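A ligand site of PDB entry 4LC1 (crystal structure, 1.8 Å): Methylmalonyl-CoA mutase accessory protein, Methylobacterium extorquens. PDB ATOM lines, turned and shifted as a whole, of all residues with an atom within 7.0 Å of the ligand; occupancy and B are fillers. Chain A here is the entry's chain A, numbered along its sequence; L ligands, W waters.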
ATOM      1  N   GLY A  62     -24.824  -7.966  14.139  1.00  0.00           N
ATOM      2  CA  GLY A  62     -25.674  -6.785  14.173  1.00  0.00           C
ATOM      3  C   GLY A  62     -24.774  -5.590  13.920  1.00  0.00           C
ATOM      4  O   GLY A  62     -23.560  -5.714  13.998  1.00  0.00           O
ATOM      5  N   VAL A  63     -25.356  -4.466  13.544  1.00  0.00           N
ATOM      6  CA  VAL A  63     -24.547  -3.283  13.193  1.00  0.00           C
ATOM      7  C   VAL A  63     -23.763  -2.760  14.397  1.00  0.00           C
ATOM      8  O   VAL A  63     -24.158  -2.956  15.523  1.00  0.00           O
ATOM      9  CB  VAL A  63     -25.425  -2.138  12.620  1.00  0.00           C
ATOM     10  CG1 VAL A  63     -26.034  -2.592  11.305  1.00  0.00           C
ATOM     11  CG2 VAL A  63     -26.470  -1.698  13.641  1.00  0.00           C
ATOM     12  N   PRO A  64     -22.631  -2.053  14.170  1.00  0.00           N
ATOM     13  CA  PRO A  64     -21.942  -1.493  15.323  1.00  0.00           C
ATOM     14  C   PRO A  64     -22.878  -0.605  16.175  1.00  0.00           C
ATOM     15  O   PRO A  64     -23.655   0.211  15.607  1.00  0.00           O
ATOM     16  CB  PRO A  64     -20.776  -0.705  14.702  1.00  0.00           C
ATOM     17  CG  PRO A  64     -20.609  -1.271  13.346  1.00  0.00           C
ATOM     18  CD  PRO A  64     -21.984  -1.695  12.906  1.00  0.00           C
ATOM     19  N   GLY A  65     -22.839  -0.781  17.496  1.00  0.00           N
ATOM     20  CA  GLY A  65     -23.704  -0.049  18.435  1.00  0.00           C
ATOM     21  C   GLY A  65     -25.115  -0.594  18.696  1.00  0.00           C
ATOM     22  O   GLY A  65     -25.878  -0.004  19.480  1.00  0.00           O
ATOM     23  N   VAL A  66     -25.461  -1.738  18.086  1.00  0.00           N
ATOM     24  CA  VAL A  66     -26.774  -2.371  18.309  1.00  0.00           C
ATOM     25  C   VAL A  66     -26.940  -2.941  19.732  1.00  0.00           C
ATOM     26  O   VAL A  66     -28.051  -3.077  20.222  1.00  0.00           O
ATOM     27  CB  VAL A  66     -27.046  -3.466  17.249  1.00  0.00           C
ATOM     28  CG1 VAL A  66     -26.138  -4.674  17.429  1.00  0.00           C
ATOM     29  CG2 VAL A  66     -28.513  -3.879  17.198  1.00  0.00           C
ATOM     30  N   GLY A  67     -25.827  -3.235  20.388  1.00  0.00           N
ATOM     31  CA  GLY A  67     -25.835  -3.844  21.720  1.00  0.00           C
ATOM     32  C   GLY A  67     -25.407  -5.297  21.734  1.00  0.00           C
ATOM     33  O   GLY A  67     -25.772  -6.021  22.643  1.00  0.00           O
ATOM     34  N   LYS A  68     -24.606  -5.718  20.769  1.00  0.00           N
ATOM     35  CA  LYS A  68     -24.192  -7.110  20.658  1.00  0.00           C
ATOM     36  C   LYS A  68     -23.340  -7.541  21.855  1.00  0.00           C
ATOM     37  O   LYS A  68     -23.623  -8.566  22.456  1.00  0.00           O
ATOM     38  CB  LYS A  68     -23.407  -7.325  19.363  1.00  0.00           C
ATOM     39  CG  LYS A  68     -22.846  -8.718  19.209  1.00  0.00           C
ATOM     40  CD  LYS A  68     -22.690  -9.094  17.743  1.00  0.00           C
ATOM     41  CE  LYS A  68     -21.693  -8.185  17.038  1.00  0.00           C
ATOM     42  NZ  LYS A  68     -20.350  -8.164  17.694  1.00  0.00           N
ATOM     43  N   SER A  69     -22.335  -6.759  22.220  1.00  0.00           N
ATOM     44  CA  SER A  69     -21.504  -7.081  23.417  1.00  0.00           C
ATOM     45  C   SER A  69     -22.328  -7.220  24.677  1.00  0.00           C
ATOM     46  O   SER A  69     -22.194  -8.145  25.440  1.00  0.00           O
ATOM     47  CB  SER A  69     -20.482  -5.964  23.670  1.00  0.00           C
ATOM     48  OG  SER A  69     -19.608  -5.883  22.583  1.00  0.00           O
ATOM     49  N   THR A  70     -23.187  -6.254  24.887  1.00  0.00           N
ATOM     50  CA  THR A  70     -24.041  -6.232  26.060  1.00  0.00           C
ATOM     51  C   THR A  70     -24.979  -7.423  26.094  1.00  0.00           C
ATOM     52  O   THR A  70     -25.193  -8.010  27.129  1.00  0.00           O
ATOM     53  CB  THR A  70     -24.847  -4.900  26.091  1.00  0.00           C
ATOM     54  OG1 THR A  70     -23.954  -3.775  26.026  1.00  0.00           O
ATOM     55  CG2 THR A  70     -25.709  -4.816  27.317  1.00  0.00           C
ATOM     56  N   THR A  71     -25.564  -7.779  24.943  1.00  0.00           N
ATOM     57  CA  THR A  71     -26.503  -8.890  24.859  1.00  0.00           C
ATOM     58  C   THR A  71     -25.798 -10.215  25.061  1.00  0.00           C
ATOM     59  O   THR A  71     -26.306 -11.069  25.745  1.00  0.00           O
ATOM     60  CB  THR A  71     -27.255  -8.902  23.504  1.00  0.00           C
ATOM     61  OG1 THR A  71     -27.996  -7.694  23.387  1.00  0.00           O
ATOM     62  CG2 THR A  71     -28.223 -10.038  23.400  1.00  0.00           C
ATOM     63  N   ILE A  72     -24.625 -10.380  24.469  1.00  0.00           N
ATOM     64  CA  ILE A  72     -23.851 -11.603  24.700  1.00  0.00           C
ATOM     65  C   ILE A  72     -23.424 -11.705  26.148  1.00  0.00           C
ATOM     66  O   ILE A  72     -23.514 -12.768  26.758  1.00  0.00           O
ATOM     67  CB  ILE A  72     -22.623 -11.672  23.776  1.00  0.00           C
ATOM     68  CG1 ILE A  72     -23.085 -11.796  22.334  1.00  0.00           C
ATOM     69  CG2 ILE A  72     -21.718 -12.839  24.158  1.00  0.00           C
ATOM     70  CD1 ILE A  72     -21.969 -11.818  21.329  1.00  0.00           C
ATOM     71  N   ARG A 108     -15.225  -5.061  27.084  1.00  0.00           N
ATOM     72  CA  ARG A 108     -16.634  -5.230  26.755  1.00  0.00           C
ATOM     73  C   ARG A 108     -16.902  -6.660  27.246  1.00  0.00           C
ATOM     74  O   ARG A 108     -15.964  -7.404  27.455  1.00  0.00           O
ATOM     75  CB  ARG A 108     -16.894  -5.050  25.252  1.00  0.00           C
ATOM     76  CG  ARG A 108     -16.109  -5.982  24.353  1.00  0.00           C
ATOM     77  CD  ARG A 108     -16.325  -5.684  22.878  1.00  0.00           C
ATOM     78  NE  ARG A 108     -15.824  -6.809  22.077  1.00  0.00           N
ATOM     79  CZ  ARG A 108     -16.560  -7.758  21.494  1.00  0.00           C
ATOM     80  NH1 ARG A 108     -15.924  -8.717  20.846  1.00  0.00           N
ATOM     81  NH2 ARG A 108     -17.903  -7.761  21.523  1.00  0.00           N
ATOM     82  N   GLU A 154     -19.322 -14.420  17.303  1.00  0.00           N
ATOM     83  CA  GLU A 154     -19.783 -13.066  16.984  1.00  0.00           C
ATOM     84  C   GLU A 154     -18.958 -12.392  15.870  1.00  0.00           C
ATOM     85  O   GLU A 154     -17.749 -12.586  15.746  1.00  0.00           O
ATOM     86  CB  GLU A 154     -19.814 -12.222  18.252  1.00  0.00           C
ATOM     87  CG  GLU A 154     -18.468 -11.990  18.860  1.00  0.00           C
ATOM     88  CD  GLU A 154     -18.366 -10.746  19.735  1.00  0.00           C
ATOM     89  OE1 GLU A 154     -19.198  -9.792  19.640  1.00  0.00           O
ATOM     90  OE2 GLU A 154     -17.397 -10.750  20.508  1.00  0.00           O
ATOM     91  N   LEU A 175     -29.220  -9.229  15.453  1.00  0.00           N
ATOM     92  CA  LEU A 175     -29.704  -8.179  16.342  1.00  0.00           C
ATOM     93  C   LEU A 175     -29.955  -6.936  15.505  1.00  0.00           C
ATOM     94  O   LEU A 175     -29.122  -6.585  14.671  1.00  0.00           O
ATOM     95  CB  LEU A 175     -28.687  -7.835  17.421  1.00  0.00           C
ATOM     96  CG  LEU A 175     -28.174  -9.019  18.253  1.00  0.00           C
ATOM     97  CD1 LEU A 175     -27.199  -8.527  19.309  1.00  0.00           C
ATOM     98  CD2 LEU A 175     -29.320  -9.776  18.907  1.00  0.00           C
ATOM     99  N   ASN A 201     -33.187  -5.149  19.703  1.00  0.00           N
ATOM    100  CA  ASN A 201     -32.617  -4.840  21.027  1.00  0.00           C
ATOM    101  C   ASN A 201     -32.996  -3.434  21.477  1.00  0.00           C
ATOM    102  O   ASN A 201     -33.574  -2.675  20.706  1.00  0.00           O
ATOM    103  CB  ASN A 201     -31.097  -5.003  21.000  1.00  0.00           C
ATOM    104  CG  ASN A 201     -30.464  -4.951  22.374  1.00  0.00           C
ATOM    105  OD1 ASN A 201     -31.030  -5.436  23.348  1.00  0.00           O
ATOM    106  ND2 ASN A 201     -29.276  -4.359  22.459  1.00  0.00           N
ATOM    107  N   LYS A 202     -32.656  -3.108  22.731  1.00  0.00           N
ATOM    108  CA  LYS A 202     -32.939  -1.784  23.348  1.00  0.00           C
ATOM    109  C   LYS A 202     -34.450  -1.562  23.570  1.00  0.00           C
ATOM    110  O   LYS A 202     -34.920  -0.416  23.554  1.00  0.00           O
ATOM    111  CB  LYS A 202     -32.266  -0.624  22.623  1.00  0.00           C
ATOM    112  CG  LYS A 202     -30.789  -0.848  22.273  1.00  0.00           C
ATOM    113  CD  LYS A 202     -30.042   0.420  21.895  1.00  0.00           C
ATOM    114  CE  LYS A 202     -28.608   0.081  21.546  1.00  0.00           C
ATOM    115  NZ  LYS A 202     -27.782   1.277  21.321  1.00  0.00           N
ATOM    116  N   ALA A 203     -35.150  -2.664  23.810  1.00  0.00           N
ATOM    117  CA  ALA A 203     -36.590  -2.687  24.097  1.00  0.00           C
ATOM    118  C   ALA A 203     -36.778  -2.408  25.611  1.00  0.00           C
ATOM    119  O   ALA A 203     -37.367  -3.201  26.349  1.00  0.00           O
ATOM    120  CB  ALA A 203     -37.224  -4.007  23.676  1.00  0.00           C
ATOM    121  N   ASP A 204     -36.224  -1.290  26.044  1.00  0.00           N
ATOM    122  CA  ASP A 204     -36.295  -0.882  27.458  1.00  0.00           C
ATOM    123  C   ASP A 204     -37.749  -0.554  27.816  1.00  0.00           C
ATOM    124  O   ASP A 204     -38.509  -0.096  26.971  1.00  0.00           O
ATOM    125  CB  ASP A 204     -35.458   0.355  27.727  1.00  0.00           C
ATOM    126  CG  ASP A 204     -33.985   0.179  27.395  1.00  0.00           C
ATOM    127  OD1 ASP A 204     -33.539  -0.886  26.946  1.00  0.00           O
ATOM    128  OD2 ASP A 204     -33.248   1.145  27.588  1.00  0.00           O
ATOM    129  N   ILE A 240     -35.921  -7.597  22.763  1.00  0.00           N
ATOM    130  CA  ILE A 240     -35.127  -7.849  23.963  1.00  0.00           C
ATOM    131  C   ILE A 240     -34.501  -6.571  24.457  1.00  0.00           C
ATOM    132  O   ILE A 240     -34.390  -5.573  23.717  1.00  0.00           O
ATOM    133  CB  ILE A 240     -33.970  -8.863  23.677  1.00  0.00           C
ATOM    134  CG1 ILE A 240     -33.001  -8.310  22.632  1.00  0.00           C
ATOM    135  CG2 ILE A 240     -34.510 -10.220  23.293  1.00  0.00           C
ATOM    136  CD1 ILE A 240     -31.767  -9.207  22.473  1.00  0.00           C
ATOM    137  N   SER A 241     -34.002  -6.631  25.705  1.00  0.00           N
ATOM    138  CA  SER A 241     -33.084  -5.633  26.220  1.00  0.00           C
ATOM    139  C   SER A 241     -31.878  -6.323  26.814  1.00  0.00           C
ATOM    140  O   SER A 241     -31.973  -6.912  27.912  1.00  0.00           O
ATOM    141  CB  SER A 241     -33.745  -4.742  27.290  1.00  0.00           C
ATOM    142  OG  SER A 241     -32.800  -3.861  27.870  1.00  0.00           O
ATOM    143  N   GLY A 242     -30.777  -6.335  26.078  1.00  0.00           N
ATOM    144  CA  GLY A 242     -29.560  -6.943  26.589  1.00  0.00           C
ATOM    145  C   GLY A 242     -29.141  -6.222  27.861  1.00  0.00           C
ATOM    146  O   GLY A 242     -28.714  -6.854  28.845  1.00  0.00           O
ATOM    147  N   LEU A 243     -29.322  -4.903  27.882  1.00  0.00           N
ATOM    148  CA  LEU A 243     -28.859  -4.109  29.015  1.00  0.00           C
ATOM    149  C   LEU A 243     -29.661  -4.446  30.266  1.00  0.00           C
ATOM    150  O   LEU A 243     -29.069  -4.573  31.354  1.00  0.00           O
ATOM    151  CB  LEU A 243     -28.885  -2.620  28.679  1.00  0.00           C
ATOM    152  CG  LEU A 243     -28.317  -1.679  29.746  1.00  0.00           C
ATOM    153  CD1 LEU A 243     -26.809  -1.850  29.881  1.00  0.00           C
ATOM    154  CD2 LEU A 243     -28.678  -0.252  29.372  1.00  0.00           C
ATOM    155  N   HIS A 244     -30.980  -4.596  30.148  1.00  0.00           N
ATOM    156  CA  HIS A 244     -31.811  -4.805  31.313  1.00  0.00           C
ATOM    157  C   HIS A 244     -32.323  -6.180  31.512  1.00  0.00           C
ATOM    158  O   HIS A 244     -33.119  -6.438  32.431  1.00  0.00           O
ATOM    159  CB  HIS A 244     -32.909  -3.754  31.335  1.00  0.00           C
ATOM    160  CG  HIS A 244     -32.339  -2.366  31.461  1.00  0.00           C
ATOM    161  ND1 HIS A 244     -31.527  -2.003  32.483  1.00  0.00           N
ATOM    162  CD2 HIS A 244     -32.434  -1.265  30.631  1.00  0.00           C
ATOM    163  CE1 HIS A 244     -31.137  -0.732  32.320  1.00  0.00           C
ATOM    164  NE2 HIS A 244     -31.695  -0.277  31.191  1.00  0.00           N
ATOM    165  N   GLY A 245     -31.839  -7.104  30.699  1.00  0.00           N
ATOM    166  CA  GLY A 245     -32.167  -8.513  30.863  1.00  0.00           C
ATOM    167  C   GLY A 245     -33.631  -8.845  30.644  1.00  0.00           C
ATOM    168  O   GLY A 245     -34.229  -9.559  31.448  1.00  0.00           O
HETATM  169  P1  LIG L   1     -22.007  -3.398  20.063  1.00  0.00           P
HETATM  170  O1  LIG L   1     -21.186  -2.377  19.317  1.00  0.00           O
HETATM  171  O2  LIG L   1     -23.152  -3.933  19.195  1.00  0.00           O
HETATM  172  O3  LIG L   1     -21.182  -4.491  20.725  1.00  0.00           O
HETATM  173  O4  LIG L   1     -22.810  -2.603  21.175  1.00  0.00           O
HETATM  174  P2  LIG L   1     -22.551  -2.535  22.777  1.00  0.00           P
HETATM  175  O5  LIG L   1     -21.149  -1.980  22.962  1.00  0.00           O
HETATM  176  O6  LIG L   1     -22.994  -3.766  23.519  1.00  0.00           O
HETATM  177  O7  LIG L   1     -23.585  -1.389  23.211  1.00  0.00           O
HETATM  178  C1  LIG L   1     -23.525  -0.107  22.582  1.00  0.00           C
HETATM  179  C2  LIG L   1     -24.246   0.900  23.461  1.00  0.00           C
HETATM  180  O8  LIG L   1     -25.640   0.596  23.502  1.00  0.00           O
HETATM  181  C3  LIG L   1     -23.763   0.880  24.904  1.00  0.00           C
HETATM  182  O9  LIG L   1     -23.781   2.196  25.456  1.00  0.00           O
HETATM  183  C4  LIG L   1     -24.797   0.024  25.627  1.00  0.00           C
HETATM  184  O10 LIG L   1     -24.941   0.308  27.021  1.00  0.00           O
HETATM  185  C5  LIG L   1     -26.041   0.348  24.829  1.00  0.00           C
HETATM  186  N1  LIG L   1     -26.967  -0.786  24.938  1.00  0.00           N
HETATM  187  C6  LIG L   1     -26.743  -2.073  24.666  1.00  0.00           C
HETATM  188  N2  LIG L   1     -27.851  -2.795  24.921  1.00  0.00           N
HETATM  189  C7  LIG L   1     -28.822  -1.946  25.323  1.00  0.00           C
HETATM  190  C8  LIG L   1     -30.227  -2.038  25.712  1.00  0.00           C
HETATM  191  O11 LIG L   1     -30.860  -3.121  25.774  1.00  0.00           O
HETATM  192  N3  LIG L   1     -30.830  -0.888  26.073  1.00  0.00           N
HETATM  193  C9  LIG L   1     -30.198   0.318  26.032  1.00  0.00           C
HETATM  194  N4  LIG L   1     -30.849   1.450  26.380  1.00  0.00           N
HETATM  195  N5  LIG L   1     -28.923   0.468  25.668  1.00  0.00           N
HETATM  196  C10 LIG L   1     -28.215  -0.617  25.318  1.00  0.00           C
HETATM  197  O   HOH W   1     -25.980   4.178  24.254  1.00  0.00           O
HETATM  198  O   HOH W   2     -18.847  -2.630  17.766  1.00  0.00           O
HETATM  199  O   HOH W   3     -19.519  -5.976  19.266  1.00  0.00           O
HETATM  200  O   HOH W   4     -18.411  -3.336  21.893  1.00  0.00           O
HETATM  201  O   HOH W   5     -23.327  -2.005  28.276  1.00  0.00           O
HETATM  202  O   HOH W   6     -22.436  -5.005  16.825  1.00  0.00           O
HETATM  203  O   HOH W   7     -28.164   2.784  23.861  1.00  0.00           O
HETATM  204  O   HOH W   8     -26.225   2.583  28.097  1.00  0.00           O
HETATM  205  O   HOH W   9     -20.367   0.306  20.271  1.00  0.00           O
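The backbone NH (N) of Leu 243 sits at hydrogen-bond distance from an oxygen (O11) of the ligand, at 3.2 Å. N2 of the ligand is in hydrogen-bond range of ND2 of Asn 201 (3.2 Å). The backbone NH (N) of Gly 242 sits at hydrogen-bond distance from an oxygen (O11) of the ligand (3.2 Å). O2 of the ligand lies within hydrogen-bond range of N of Val 66. The side-chain hydroxyl (OG1) of Thr 70 lies within hydrogen-bond range of an oxygen (O6) of the ligand (2.7 Å). The backbone NH of Gly 65 lies within hydrogen-bond range of an oxygen (O1) of the ligand. OD2 of Asp 204 is in hydrogen-bond range of N4 of the ligand. An oxygen (O11) of the ligand is in hydrogen-bond range of the side-chain hydroxyl (OG) of Ser 241 (3.0 Å). The side-chain hydroxyl (OG) of Ser 69 lies within hydrogen-bond range of an oxygen (O3) of the ligand, at 2.8 Å. An oxygen (O2) of the ligand lies within hydrogen-bond range of the backbone NH of Gly 67 (3.0 Å). N of Thr 70 lies within hydrogen-bond range of O6 of the ligand, 2.8 Å away. The backbone NH (N) of Lys 68 lies within hydrogen-bond range of an oxygen (O2) of the ligand, 2.8 Å away. N of Ser 69 is in hydrogen-bond range of O3 of the ligand, 3.0 Å away. An oxygen (O8) of the ligand is in hydrogen-bond range of the side-chain amino group of Lys 202 (3.1 Å).
Water W3 lies within hydrogen-bond range of an oxygen (O3) of the ligand (2.7 Å), the side-chain amino group (NZ) of Lys 68 (2.8 Å), the guanidinium group (NH2) of Arg 108 (3.3 Å) and the side-chain hydroxyl (OG) of Ser 69 (3.3 Å). Water W6 lies within hydrogen-bond range of an oxygen (O2) of the ligand (2.7 Å), the backbone carbonyl oxygen (O) of Val 63 (3.0 Å) and the backbone carbonyl oxygen (O) of Gly 62 (3.1 Å). Water W7 bridges the side-chain amino group of Lys 202 (3.0 Å) and a nitrogen (N5) of the ligand (3.0 Å). Water W5 lies within hydrogen-bond range of the side-chain hydroxyl of Thr 70 (2.9 Å) and an oxygen (O10) of the ligand (3.1 Å). Water W4 lies within hydrogen-bond range of the side-chain hydroxyl of Ser 69 and an oxygen (O3) of the ligand.
Val 63 touches the ligand. C of Pro 64 touches O1 of the ligand (3.98 Å). Of the 24 residues printed, 14 come within 4 Å of the ligand.
The backbone carbonyl oxygen (O) of Gly 67 is in hydrogen-bond range of the side-chain hydroxyl (OG1) of Thr 71, 2.9 Å away. OG of Ser 241 lies within hydrogen-bond range of N of His 244 (3.0 Å). The backbone NH (N) of Gly 242 is in hydrogen-bond range of the side-chain amide oxygen (OD1) of Asn 201 (2.9 Å). The backbone carbonyl oxygen of Val 66 is in hydrogen-bond range of the side-chain amide nitrogen of Asn 201, at 2.9 Å. The side-chain amide oxygen of Asn 201 lies close to the backbone carbonyl oxygen of Ile 240. O of Gly 65 sits at hydrogen-bond distance from NZ of Lys 202, at 2.9 Å. OD1 of Asp 204 is in hydrogen-bond range of OG of Ser 241, 3.2 Å away. O of Ile 240 lies within hydrogen-bond range of N of Lys 202, at 3.2 Å.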
